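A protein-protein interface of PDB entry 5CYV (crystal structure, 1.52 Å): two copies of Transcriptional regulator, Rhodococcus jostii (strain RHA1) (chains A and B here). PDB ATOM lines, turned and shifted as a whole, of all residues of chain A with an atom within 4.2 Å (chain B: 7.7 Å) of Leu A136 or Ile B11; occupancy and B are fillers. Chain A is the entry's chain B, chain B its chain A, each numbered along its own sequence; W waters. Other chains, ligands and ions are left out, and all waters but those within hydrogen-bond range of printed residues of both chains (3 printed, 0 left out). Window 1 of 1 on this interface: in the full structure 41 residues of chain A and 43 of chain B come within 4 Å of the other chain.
Among the printed residues, pairs that only touch across the chains: Phe A121 with Leu B15, Thr A135 with Val B128, Arg A133 with Ile B11, Leu A15 with Gly B19, Gln A137 with Leu B14, Leu A136 with Leu B15, Met A132 with Ile B11, Arg A133 with Leu B14, Phe A121 with Ile B11, Thr A135 with Ile B124, Leu A15 with Phe B121, Phe A121 with Gly B12, Ile A139 with Phe B121, Thr A135 with Met B132, Leu A136 with Val B18, Ile A139 with Met B21, Leu A15 with Leu B136, Leu A136 with Ile B11, Ile A139 with Ile B124, Leu A15 with Leu B15, Leu A15 with Met B132, Ala A140 with Met B21 and Leu A136 with Leu B14.
Leu B15 touches its own counterpart, Leu A15.
Leu A15 touches Phe B121, and with the chains exchanged Phe A121 touches Leu B15.
Leu A15 touches Leu B136, and with the chains exchanged Leu A136 touches Leu B15.
Ile A139 touches Phe B121, but with the chains exchanged Phe A121 does not touch Ile B139 (4.2 Å).
OD2 of Asp B10 sits at hydrogen-bond distance from N of Gly B12 (3.0 Å).
The backbone carbonyl oxygen (O) of Gly B12 is in hydrogen-bond range of the side-chain hydroxyl (OG) of Ser B16 (3.2 Å).
OG of Ser A138 lies within hydrogen-bond range of O of Thr A135.
The side-chain hydroxyl (OG) of Ser B4 sits at hydrogen-bond distance from the side-chain carboxylate (OD2) of Asp B9, 2.6 Å away.
Of the 11 printed residues of chain A, 9 touch a printed residue of chain B.
Printed residues of chain A that touch a printed residue of chain B: Leu A15, Phe A121, Met A132, Arg A133, Thr A135, Leu A136, Gln A137, Ile A139 and Ala A140.
Hydrophobic or aromatic side chains of chain A within 4 Å of the printed part of chain B: Leu A15, Phe A121, Met A132, Leu A136 and Ile A139.
Hydrophobic or aromatic side chains of chain B that line the printed part of chain A: Ile B11, Leu B14, Leu B15, Val B18, Met B21, Phe B121, Ile B124, Val B128, Met B132 and Leu B136.
Along chain B the printed residues that touch a printed residue of chain A span positions 8 to 136.
Among the printed residues, 26 pairs touch across the chains.
NE2 of Gln A137 is in hydrogen-bond range of OD1 of Asp B9 (2.8 Å).
O of Asp B9 sits at hydrogen-bond distance from NE of Arg A133 (2.9 Å).
The backbone carbonyl oxygen of Ser B8 is in hydrogen-bond range of the side-chain amide nitrogen of Gln A137.
Water W3 lies within hydrogen-bond range of the guanidinium group (NH1) of Arg B17 and the backbone carbonyl oxygen (O) of Ala A140.
Water W2 lies within hydrogen-bond range of OG of Ser B8 (2.7 Å), OD1 of Asp B9 (2.7 Å) and NE2 of Gln A137 (3.4 Å).
Water W1 lies within hydrogen-bond range of NH2 of Arg A133 (2.9 Å), N of Ile B11 (3.0 Å) and O of Asp B9 (3.4 Å).
Of chain B, only Ile B11 (3.8 Å), Leu B14 (3.9 Å), Leu B15 (3.7 Å) and Val B18 (3.8 Å) come within 4 Å of Leu A136.
Of the printed residues of chain B, Gln A137 touches Ser B8 (3.0 Å), Asp B9 (2.8 Å) and Leu B14 (3.6 Å).
Leu B7 touches none of the printed residues of chain A.
Asp B10 touches none of the printed residues of chain A.
Of chain A, only Phe A121 (3.7 Å), Met A132 (3.7 Å), Arg A133 (3.6 Å) and Leu A136 (3.8 Å) come within 4 Å of Ile B11.
Printed residues of chain A within 4 Å of Val B18: Leu A136 (3.8 Å).
The nearest residue of chain B that does not touch Leu A136 is Met B132 (4.3 Å).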
ATOM      1  N   LEU A  15      23.311  37.220  27.057  1.00  0.00           N
ATOM      2  CA  LEU A  15      23.503  35.829  27.481  1.00  0.00           C
ATOM      3  C   LEU A  15      23.457  35.736  28.996  1.00  0.00           C
ATOM      4  O   LEU A  15      22.824  34.814  29.551  1.00  0.00           O
ATOM      5  CB  LEU A  15      24.818  35.302  26.942  1.00  0.00           C
ATOM      6  CG  LEU A  15      24.740  34.974  25.428  1.00  0.00           C
ATOM      7  CD1 LEU A  15      26.176  34.917  24.848  1.00  0.00           C
ATOM      8  CD2 LEU A  15      23.976  33.644  25.077  1.00  0.00           C
ATOM      9  N   PHE A 121      10.916  29.840  26.442  1.00  0.00           N
ATOM     10  CA  PHE A 121      11.322  29.233  25.150  1.00  0.00           C
ATOM     11  C   PHE A 121      10.202  28.686  24.308  1.00  0.00           C
ATOM     12  O   PHE A 121      10.407  28.472  23.112  1.00  0.00           O
ATOM     13  CB  PHE A 121      12.317  28.103  25.366  1.00  0.00           C
ATOM     14  CG  PHE A 121      13.493  28.483  26.209  1.00  0.00           C
ATOM     15  CD1 PHE A 121      14.306  29.551  25.824  1.00  0.00           C
ATOM     16  CD2 PHE A 121      13.791  27.787  27.344  1.00  0.00           C
ATOM     17  CE1 PHE A 121      15.379  29.904  26.604  1.00  0.00           C
ATOM     18  CE2 PHE A 121      14.873  28.164  28.138  1.00  0.00           C
ATOM     19  CZ  PHE A 121      15.647  29.202  27.754  1.00  0.00           C
ATOM     20  N   MET A 132      20.146  28.396  18.004  1.00  0.00           N
ATOM     21  CA  MET A 132      20.721  28.824  19.285  1.00  0.00           C
ATOM     22  C   MET A 132      21.376  27.624  20.007  1.00  0.00           C
ATOM     23  O   MET A 132      22.491  27.747  20.530  1.00  0.00           O
ATOM     24  CB  MET A 132      19.641  29.444  20.145  1.00  0.00           C
ATOM     25  CG  MET A 132      20.198  29.986  21.398  1.00  0.00           C
ATOM     26  SD  MET A 132      19.044  31.192  22.112  1.00  0.00           S
ATOM     27  CE  MET A 132      18.830  32.200  20.676  1.00  0.00           C
ATOM     28  N   ARG A 133      20.657  26.498  20.053  1.00  0.00           N
ATOM     29  CA  ARG A 133      21.186  25.301  20.741  1.00  0.00           C
ATOM     30  C   ARG A 133      22.539  24.936  20.197  1.00  0.00           C
ATOM     31  O   ARG A 133      23.524  24.746  20.930  1.00  0.00           O
ATOM     32  CB  ARG A 133      20.245  24.101  20.567  1.00  0.00           C
ATOM     33  CG  ARG A 133      20.787  22.820  21.270  1.00  0.00           C
ATOM     34  CD  ARG A 133      19.903  21.601  21.016  1.00  0.00           C
ATOM     35  NE  ARG A 133      18.590  21.875  21.567  1.00  0.00           N
ATOM     36  CZ  ARG A 133      17.479  22.120  20.860  1.00  0.00           C
ATOM     37  NH1 ARG A 133      17.507  22.185  19.511  1.00  0.00           N
ATOM     38  NH2 ARG A 133      16.344  22.341  21.519  1.00  0.00           N
ATOM     39  N   ASP A 134      22.629  24.798  18.882  1.00  0.00           N
ATOM     40  CA  ASP A 134      23.843  24.322  18.279  1.00  0.00           C
ATOM     41  C   ASP A 134      24.956  25.343  18.470  1.00  0.00           C
ATOM     42  O   ASP A 134      26.088  24.951  18.701  1.00  0.00           O
ATOM     43  CB  ASP A 134      23.623  23.978  16.795  1.00  0.00           C
ATOM     44  CG  ASP A 134      22.696  22.772  16.599  1.00  0.00           C
ATOM     45  OD1 ASP A 134      22.157  22.224  17.608  1.00  0.00           O
ATOM     46  OD2 ASP A 134      22.480  22.404  15.428  1.00  0.00           O
ATOM     47  N   THR A 135      24.640  26.645  18.389  1.00  0.00           N
ATOM     48  CA  THR A 135      25.657  27.671  18.575  1.00  0.00           C
ATOM     49  C   THR A 135      26.176  27.638  20.025  1.00  0.00           C
ATOM     50  O   THR A 135      27.415  27.683  20.255  1.00  0.00           O
ATOM     51  CB  THR A 135      25.089  29.077  18.220  1.00  0.00           C
ATOM     52  OG1 THR A 135      24.642  29.017  16.862  1.00  0.00           O
ATOM     53  CG2 THR A 135      26.197  30.109  18.294  1.00  0.00           C
ATOM     54  N   LEU A 136      25.263  27.529  20.994  1.00  0.00           N
ATOM     55  CA  LEU A 136      25.678  27.510  22.412  1.00  0.00           C
ATOM     56  C   LEU A 136      26.492  26.229  22.667  1.00  0.00           C
ATOM     57  O   LEU A 136      27.480  26.268  23.410  1.00  0.00           O
ATOM     58  CB  LEU A 136      24.477  27.565  23.331  1.00  0.00           C
ATOM     59  CG  LEU A 136      23.706  28.890  23.214  1.00  0.00           C
ATOM     60  CD1 LEU A 136      22.453  28.688  24.024  1.00  0.00           C
ATOM     61  CD2 LEU A 136      24.498  30.071  23.773  1.00  0.00           C
ATOM     62  N   GLN A 137      26.112  25.110  22.057  1.00  0.00           N
ATOM     63  CA  GLN A 137      26.952  23.914  22.227  1.00  0.00           C
ATOM     64  C   GLN A 137      28.346  24.103  21.685  1.00  0.00           C
ATOM     65  O   GLN A 137      29.322  23.593  22.284  1.00  0.00           O
ATOM     66  CB  GLN A 137      26.298  22.724  21.558  1.00  0.00           C
ATOM     67  CG  GLN A 137      25.119  22.238  22.329  1.00  0.00           C
ATOM     68  CD  GLN A 137      24.394  21.133  21.604  1.00  0.00           C
ATOM     69  OE1 GLN A 137      24.490  21.050  20.378  1.00  0.00           O
ATOM     70  NE2 GLN A 137      23.727  20.249  22.329  1.00  0.00           N
ATOM     71  N   SER A 138      28.498  24.812  20.557  1.00  0.00           N
ATOM     72  CA  SER A 138      29.828  24.978  19.996  1.00  0.00           C
ATOM     73  C   SER A 138      30.708  25.862  20.881  1.00  0.00           C
ATOM     74  O   SER A 138      31.929  25.755  20.838  1.00  0.00           O
ATOM     75  CB  SER A 138      29.749  25.543  18.582  1.00  0.00           C
ATOM     76  OG  SER A 138      29.429  26.903  18.620  1.00  0.00           O
ATOM     77  N   ILE A 139      30.097  26.711  21.693  1.00  0.00           N
ATOM     78  CA  ILE A 139      30.821  27.543  22.640  1.00  0.00           C
ATOM     79  C   ILE A 139      31.120  26.782  23.941  1.00  0.00           C
ATOM     80  O   ILE A 139      32.279  26.763  24.405  1.00  0.00           O
ATOM     81  CB  ILE A 139      29.996  28.818  22.970  1.00  0.00           C
ATOM     82  CG1 ILE A 139      29.857  29.686  21.733  1.00  0.00           C
ATOM     83  CG2 ILE A 139      30.689  29.628  24.094  1.00  0.00           C
ATOM     84  CD1 ILE A 139      28.865  30.832  21.975  1.00  0.00           C
ATOM     85  N   ALA A 140      30.119  26.120  24.518  1.00  0.00           N
ATOM     86  CA  ALA A 140      30.350  25.413  25.785  1.00  0.00           C
ATOM     87  C   ALA A 140      31.222  24.160  25.602  1.00  0.00           C
ATOM     88  O   ALA A 140      31.998  23.797  26.519  1.00  0.00           O
ATOM     89  CB  ALA A 140      29.087  25.020  26.416  1.00  0.00           C
ATOM     90  N   SER B   4      15.758  15.093  21.786  1.00  0.00           N
ATOM     91  CA  SER B   4      16.653  14.692  22.892  1.00  0.00           C
ATOM     92  C   SER B   4      16.327  15.318  24.235  1.00  0.00           C
ATOM     93  O   SER B   4      16.204  16.545  24.366  1.00  0.00           O
ATOM     94  CB  SER B   4      18.127  15.034  22.601  1.00  0.00           C
ATOM     95  OG  SER B   4      18.927  14.875  23.797  1.00  0.00           O
ATOM     96  N   ALA B   6      18.501  14.949  26.755  1.00  0.00           N
ATOM     97  CA  ALA B   6      19.817  15.053  27.444  1.00  0.00           C
ATOM     98  C   ALA B   6      20.054  16.441  27.968  1.00  0.00           C
ATOM     99  O   ALA B   6      19.739  17.416  27.311  1.00  0.00           O
ATOM    100  CB  ALA B   6      20.956  14.717  26.527  1.00  0.00           C
ATOM    101  N   LEU B   7      20.700  16.558  29.125  1.00  0.00           N
ATOM    102  CA  LEU B   7      20.966  17.903  29.693  1.00  0.00           C
ATOM    103  C   LEU B   7      21.818  18.772  28.773  1.00  0.00           C
ATOM    104  O   LEU B   7      21.581  19.976  28.637  1.00  0.00           O
ATOM    105  CB  LEU B   7      21.634  17.755  31.080  1.00  0.00           C
ATOM    106  CG  LEU B   7      21.822  19.118  31.809  1.00  0.00           C
ATOM    107  CD1 LEU B   7      20.484  19.707  32.127  1.00  0.00           C
ATOM    108  CD2 LEU B   7      22.602  18.831  33.094  1.00  0.00           C
ATOM    109  N   SER B   8      22.775  18.120  28.102  1.00  0.00           N
ATOM    110  CA  SER B   8      23.701  18.915  27.301  1.00  0.00           C
ATOM    111  C   SER B   8      23.017  19.388  26.018  1.00  0.00           C
ATOM    112  O   SER B   8      23.585  20.231  25.325  1.00  0.00           O
ATOM    113  CB  SER B   8      24.958  18.095  26.981  1.00  0.00           C
ATOM    114  OG  SER B   8      24.684  16.968  26.197  1.00  0.00           O
ATOM    115  N   ASP B   9      21.812  18.894  25.705  1.00  0.00           N
ATOM    116  CA  ASP B   9      21.025  19.407  24.556  1.00  0.00           C
ATOM    117  C   ASP B   9      19.952  20.392  25.002  1.00  0.00           C
ATOM    118  O   ASP B   9      19.204  20.909  24.185  1.00  0.00           O
ATOM    119  CB  ASP B   9      20.344  18.257  23.823  1.00  0.00           C
ATOM    120  CG  ASP B   9      21.322  17.361  23.105  1.00  0.00           C
ATOM    121  OD1 ASP B   9      22.290  17.907  22.514  1.00  0.00           O
ATOM    122  OD2 ASP B   9      21.129  16.102  23.134  1.00  0.00           O
ATOM    123  N   ASP B  10      19.892  20.675  26.316  1.00  0.00           N
ATOM    124  CA  ASP B  10      18.775  21.481  26.796  1.00  0.00           C
ATOM    125  C   ASP B  10      19.074  22.953  26.635  1.00  0.00           C
ATOM    126  O   ASP B  10      20.087  23.414  27.128  1.00  0.00           O
ATOM    127  CB  ASP B  10      18.482  21.140  28.259  1.00  0.00           C
ATOM    128  CG  ASP B  10      17.343  21.923  28.813  1.00  0.00           C
ATOM    129  OD1 ASP B  10      16.179  21.535  28.658  1.00  0.00           O
ATOM    130  OD2 ASP B  10      17.644  22.991  29.405  1.00  0.00           O
ATOM    131  N   ILE B  11      18.219  23.704  25.981  1.00  0.00           N
ATOM    132  CA  ILE B  11      18.576  25.090  25.676  1.00  0.00           C
ATOM    133  C   ILE B  11      18.691  25.933  26.942  1.00  0.00           C
ATOM    134  O   ILE B  11      19.520  26.853  26.975  1.00  0.00           O
ATOM    135  CB  ILE B  11      17.567  25.720  24.718  1.00  0.00           C
ATOM    136  CG1 ILE B  11      18.038  27.082  24.229  1.00  0.00           C
ATOM    137  CG2 ILE B  11      16.138  25.771  25.307  1.00  0.00           C
ATOM    138  CD1 ILE B  11      19.136  26.965  23.245  1.00  0.00           C
ATOM    139  N   GLY B  12      17.869  25.632  27.954  1.00  0.00           N
ATOM    140  CA  GLY B  12      18.005  26.405  29.199  1.00  0.00           C
ATOM    141  C   GLY B  12      19.333  26.172  29.895  1.00  0.00           C
ATOM    142  O   GLY B  12      19.971  27.100  30.396  1.00  0.00           O
ATOM    143  N   PHE B  13      19.753  24.911  29.917  1.00  0.00           N
ATOM    144  CA  PHE B  13      21.040  24.578  30.514  1.00  0.00           C
ATOM    145  C   PHE B  13      22.145  25.285  29.750  1.00  0.00           C
ATOM    146  O   PHE B  13      23.060  25.898  30.334  1.00  0.00           O
ATOM    147  CB  PHE B  13      21.232  23.058  30.501  1.00  0.00           C
ATOM    148  CG  PHE B  13      22.603  22.625  30.898  1.00  0.00           C
ATOM    149  CD1 PHE B  13      22.946  22.592  32.252  1.00  0.00           C
ATOM    150  CD2 PHE B  13      23.518  22.163  29.943  1.00  0.00           C
ATOM    151  CE1 PHE B  13      24.215  22.135  32.653  1.00  0.00           C
ATOM    152  CE2 PHE B  13      24.788  21.684  30.354  1.00  0.00           C
ATOM    153  CZ  PHE B  13      25.114  21.691  31.690  1.00  0.00           C
ATOM    154  N   LEU B  14      22.059  25.199  28.419  1.00  0.00           N
ATOM    155  CA  LEU B  14      23.094  25.816  27.606  1.00  0.00           C
ATOM    156  C   LEU B  14      23.175  27.320  27.777  1.00  0.00           C
ATOM    157  O   LEU B  14      24.277  27.894  27.786  1.00  0.00           O
ATOM    158  CB  LEU B  14      22.857  25.435  26.146  1.00  0.00           C
ATOM    159  CG  LEU B  14      23.066  23.936  25.878  1.00  0.00           C
ATOM    160  CD1 LEU B  14      22.487  23.561  24.469  1.00  0.00           C
ATOM    161  CD2 LEU B  14      24.593  23.588  25.960  1.00  0.00           C
ATOM    162  N   LEU B  15      22.021  27.998  27.782  1.00  0.00           N
ATOM    163  CA  LEU B  15      22.048  29.432  27.998  1.00  0.00           C
ATOM    164  C   LEU B  15      22.614  29.815  29.347  1.00  0.00           C
ATOM    165  O   LEU B  15      23.449  30.744  29.436  1.00  0.00           O
ATOM    166  CB  LEU B  15      20.613  29.959  27.893  1.00  0.00           C
ATOM    167  CG  LEU B  15      20.191  30.212  26.492  1.00  0.00           C
ATOM    168  CD1 LEU B  15      18.671  30.417  26.416  1.00  0.00           C
ATOM    169  CD2 LEU B  15      20.930  31.485  25.916  1.00  0.00           C
ATOM    170  N   SER B  16      22.231  29.093  30.410  1.00  0.00           N
ATOM    171  CA  SER B  16      22.772  29.391  31.712  1.00  0.00           C
ATOM    172  C   SER B  16      24.245  29.122  31.759  1.00  0.00           C
ATOM    173  O   SER B  16      25.002  29.864  32.406  1.00  0.00           O
ATOM    174  CB  SER B  16      22.075  28.554  32.749  1.00  0.00           C
ATOM    175  OG  SER B  16      20.739  28.977  32.836  1.00  0.00           O
ATOM    176  N   ARG B  17      24.672  28.029  31.119  1.00  0.00           N
ATOM    177  CA  ARG B  17      26.097  27.693  31.116  1.00  0.00           C
ATOM    178  C   ARG B  17      26.911  28.718  30.352  1.00  0.00           C
ATOM    179  O   ARG B  17      27.952  29.206  30.835  1.00  0.00           O
ATOM    180  CB  ARG B  17      26.300  26.307  30.532  1.00  0.00           C
ATOM    181  CG  ARG B  17      25.898  25.216  31.530  1.00  0.00           C
ATOM    182  CD  ARG B  17      27.086  24.797  32.388  1.00  0.00           C
ATOM    183  NE  ARG B  17      28.049  24.018  31.585  1.00  0.00           N
ATOM    184  CZ  ARG B  17      29.229  24.467  31.151  1.00  0.00           C
ATOM    185  NH1 ARG B  17      29.979  23.661  30.421  1.00  0.00           N
ATOM    186  NH2 ARG B  17      29.677  25.677  31.471  1.00  0.00           N
ATOM    187  N   VAL B  18      26.476  29.074  29.159  1.00  0.00           N
ATOM    188  CA  VAL B  18      27.261  30.036  28.349  1.00  0.00           C
ATOM    189  C   VAL B  18      27.166  31.442  28.984  1.00  0.00           C
ATOM    190  O   VAL B  18      28.174  32.139  29.042  1.00  0.00           O
ATOM    191  CB  VAL B  18      26.814  30.051  26.909  1.00  0.00           C
ATOM    192  CG1 VAL B  18      27.541  31.132  26.146  1.00  0.00           C
ATOM    193  CG2 VAL B  18      27.142  28.699  26.281  1.00  0.00           C
ATOM    194  N   GLY B  19      26.020  31.766  29.581  1.00  0.00           N
ATOM    195  CA  GLY B  19      25.899  33.059  30.319  1.00  0.00           C
ATOM    196  C   GLY B  19      26.918  33.109  31.433  1.00  0.00           C
ATOM    197  O   GLY B  19      27.519  34.186  31.681  1.00  0.00           O
ATOM    198  N   MET B  21      29.786  31.358  31.663  1.00  0.00           N
ATOM    199  CA  MET B  21      31.115  31.412  31.020  1.00  0.00           C
ATOM    200  C   MET B  21      31.469  32.843  30.618  1.00  0.00           C
ATOM    201  O   MET B  21      32.579  33.325  30.860  1.00  0.00           O
ATOM    202  CB  MET B  21      31.196  30.548  29.755  1.00  0.00           C
ATOM    203  CG  MET B  21      31.143  29.053  30.089  1.00  0.00           C
ATOM    204  SD  MET B  21      30.900  28.040  28.583  1.00  0.00           S
ATOM    205  CE  MET B  21      32.419  28.486  27.770  1.00  0.00           C
ATOM    206  N   PHE B 121      33.114  34.037  20.637  1.00  0.00           N
ATOM    207  CA  PHE B 121      32.322  33.958  19.411  1.00  0.00           C
ATOM    208  C   PHE B 121      33.160  33.933  18.146  1.00  0.00           C
ATOM    209  O   PHE B 121      32.636  34.092  17.034  1.00  0.00           O
ATOM    210  CB  PHE B 121      31.317  35.105  19.329  1.00  0.00           C
ATOM    211  CG  PHE B 121      30.062  34.856  20.101  1.00  0.00           C
ATOM    212  CD1 PHE B 121      29.974  35.226  21.444  1.00  0.00           C
ATOM    213  CD2 PHE B 121      28.974  34.246  19.498  1.00  0.00           C
ATOM    214  CE1 PHE B 121      28.821  35.003  22.152  1.00  0.00           C
ATOM    215  CE2 PHE B 121      27.822  34.017  20.214  1.00  0.00           C
ATOM    216  CZ  PHE B 121      27.728  34.392  21.513  1.00  0.00           C
ATOM    217  N   ILE B 124      32.016  32.398  14.746  1.00  0.00           N
ATOM    218  CA  ILE B 124      30.556  32.499  14.664  1.00  0.00           C
ATOM    219  C   ILE B 124      30.213  33.776  13.904  1.00  0.00           C
ATOM    220  O   ILE B 124      30.563  34.855  14.304  1.00  0.00           O
ATOM    221  CB  ILE B 124      29.904  32.468  16.079  1.00  0.00           C
ATOM    222  CG1 ILE B 124      30.143  31.079  16.698  1.00  0.00           C
ATOM    223  CG2 ILE B 124      28.395  32.800  16.010  1.00  0.00           C
ATOM    224  CD1 ILE B 124      29.797  31.008  18.151  1.00  0.00           C
ATOM    225  N   VAL B 128      24.646  35.032  12.727  1.00  0.00           N
ATOM    226  CA  VAL B 128      24.192  34.200  13.856  1.00  0.00           C
ATOM    227  C   VAL B 128      24.114  35.002  15.141  1.00  0.00           C
ATOM    228  O   VAL B 128      23.126  34.876  15.887  1.00  0.00           O
ATOM    229  CB  VAL B 128      25.132  32.976  13.986  1.00  0.00           C
ATOM    230  CG1 VAL B 128      24.797  32.115  15.258  1.00  0.00           C
ATOM    231  CG2 VAL B 128      25.053  32.093  12.756  1.00  0.00           C
ATOM    232  N   MET B 132      20.752  35.668  17.432  1.00  0.00           N
ATOM    233  CA  MET B 132      20.788  35.429  18.898  1.00  0.00           C
ATOM    234  C   MET B 132      20.435  36.670  19.685  1.00  0.00           C
ATOM    235  O   MET B 132      19.647  36.582  20.657  1.00  0.00           O
ATOM    236  CB  MET B 132      22.163  34.923  19.300  1.00  0.00           C
ATOM    237  CG  MET B 132      22.321  33.495  18.839  1.00  0.00           C
ATOM    238  SD  MET B 132      23.775  32.700  19.580  1.00  0.00           S
ATOM    239  CE  MET B 132      23.786  33.434  21.219  1.00  0.00           C
ATOM    240  N   LEU B 136      17.337  36.781  22.269  1.00  0.00           N
ATOM    241  CA  LEU B 136      17.536  37.046  23.713  1.00  0.00           C
ATOM    242  C   LEU B 136      16.819  38.319  24.169  1.00  0.00           C
ATOM    243  O   LEU B 136      16.262  38.388  25.259  1.00  0.00           O
ATOM    244  CB  LEU B 136      19.027  37.144  24.064  1.00  0.00           C
ATOM    245  CG  LEU B 136      19.757  35.807  23.786  1.00  0.00           C
ATOM    246  CD1 LEU B 136      21.270  36.056  23.895  1.00  0.00           C
ATOM    247  CD2 LEU B 136      19.305  34.738  24.752  1.00  0.00           C
ATOM    248  N   ILE B 139      13.255  37.655  24.894  1.00  0.00           N
ATOM    249  CA  ILE B 139      13.031  36.954  26.178  1.00  0.00           C
ATOM    250  C   ILE B 139      13.176  37.893  27.359  1.00  0.00           C
ATOM    251  O   ILE B 139      12.316  37.930  28.239  1.00  0.00           O
ATOM    252  CB  ILE B 139      14.018  35.791  26.329  1.00  0.00           C
ATOM    253  CG1 ILE B 139      13.730  34.765  25.231  1.00  0.00           C
ATOM    254  CG2 ILE B 139      13.865  35.114  27.728  1.00  0.00           C
ATOM    255  CD1 ILE B 139      14.826  33.731  25.045  1.00  0.00           C
HETATM  256  O   HOH W   1      16.098  22.335  24.415  1.00  0.00           O
HETATM  257  O   HOH W   2      24.652  17.186  23.551  1.00  0.00           O
HETATM  258  O   HOH W   3      32.325  24.106  29.294  1.00  0.00           O
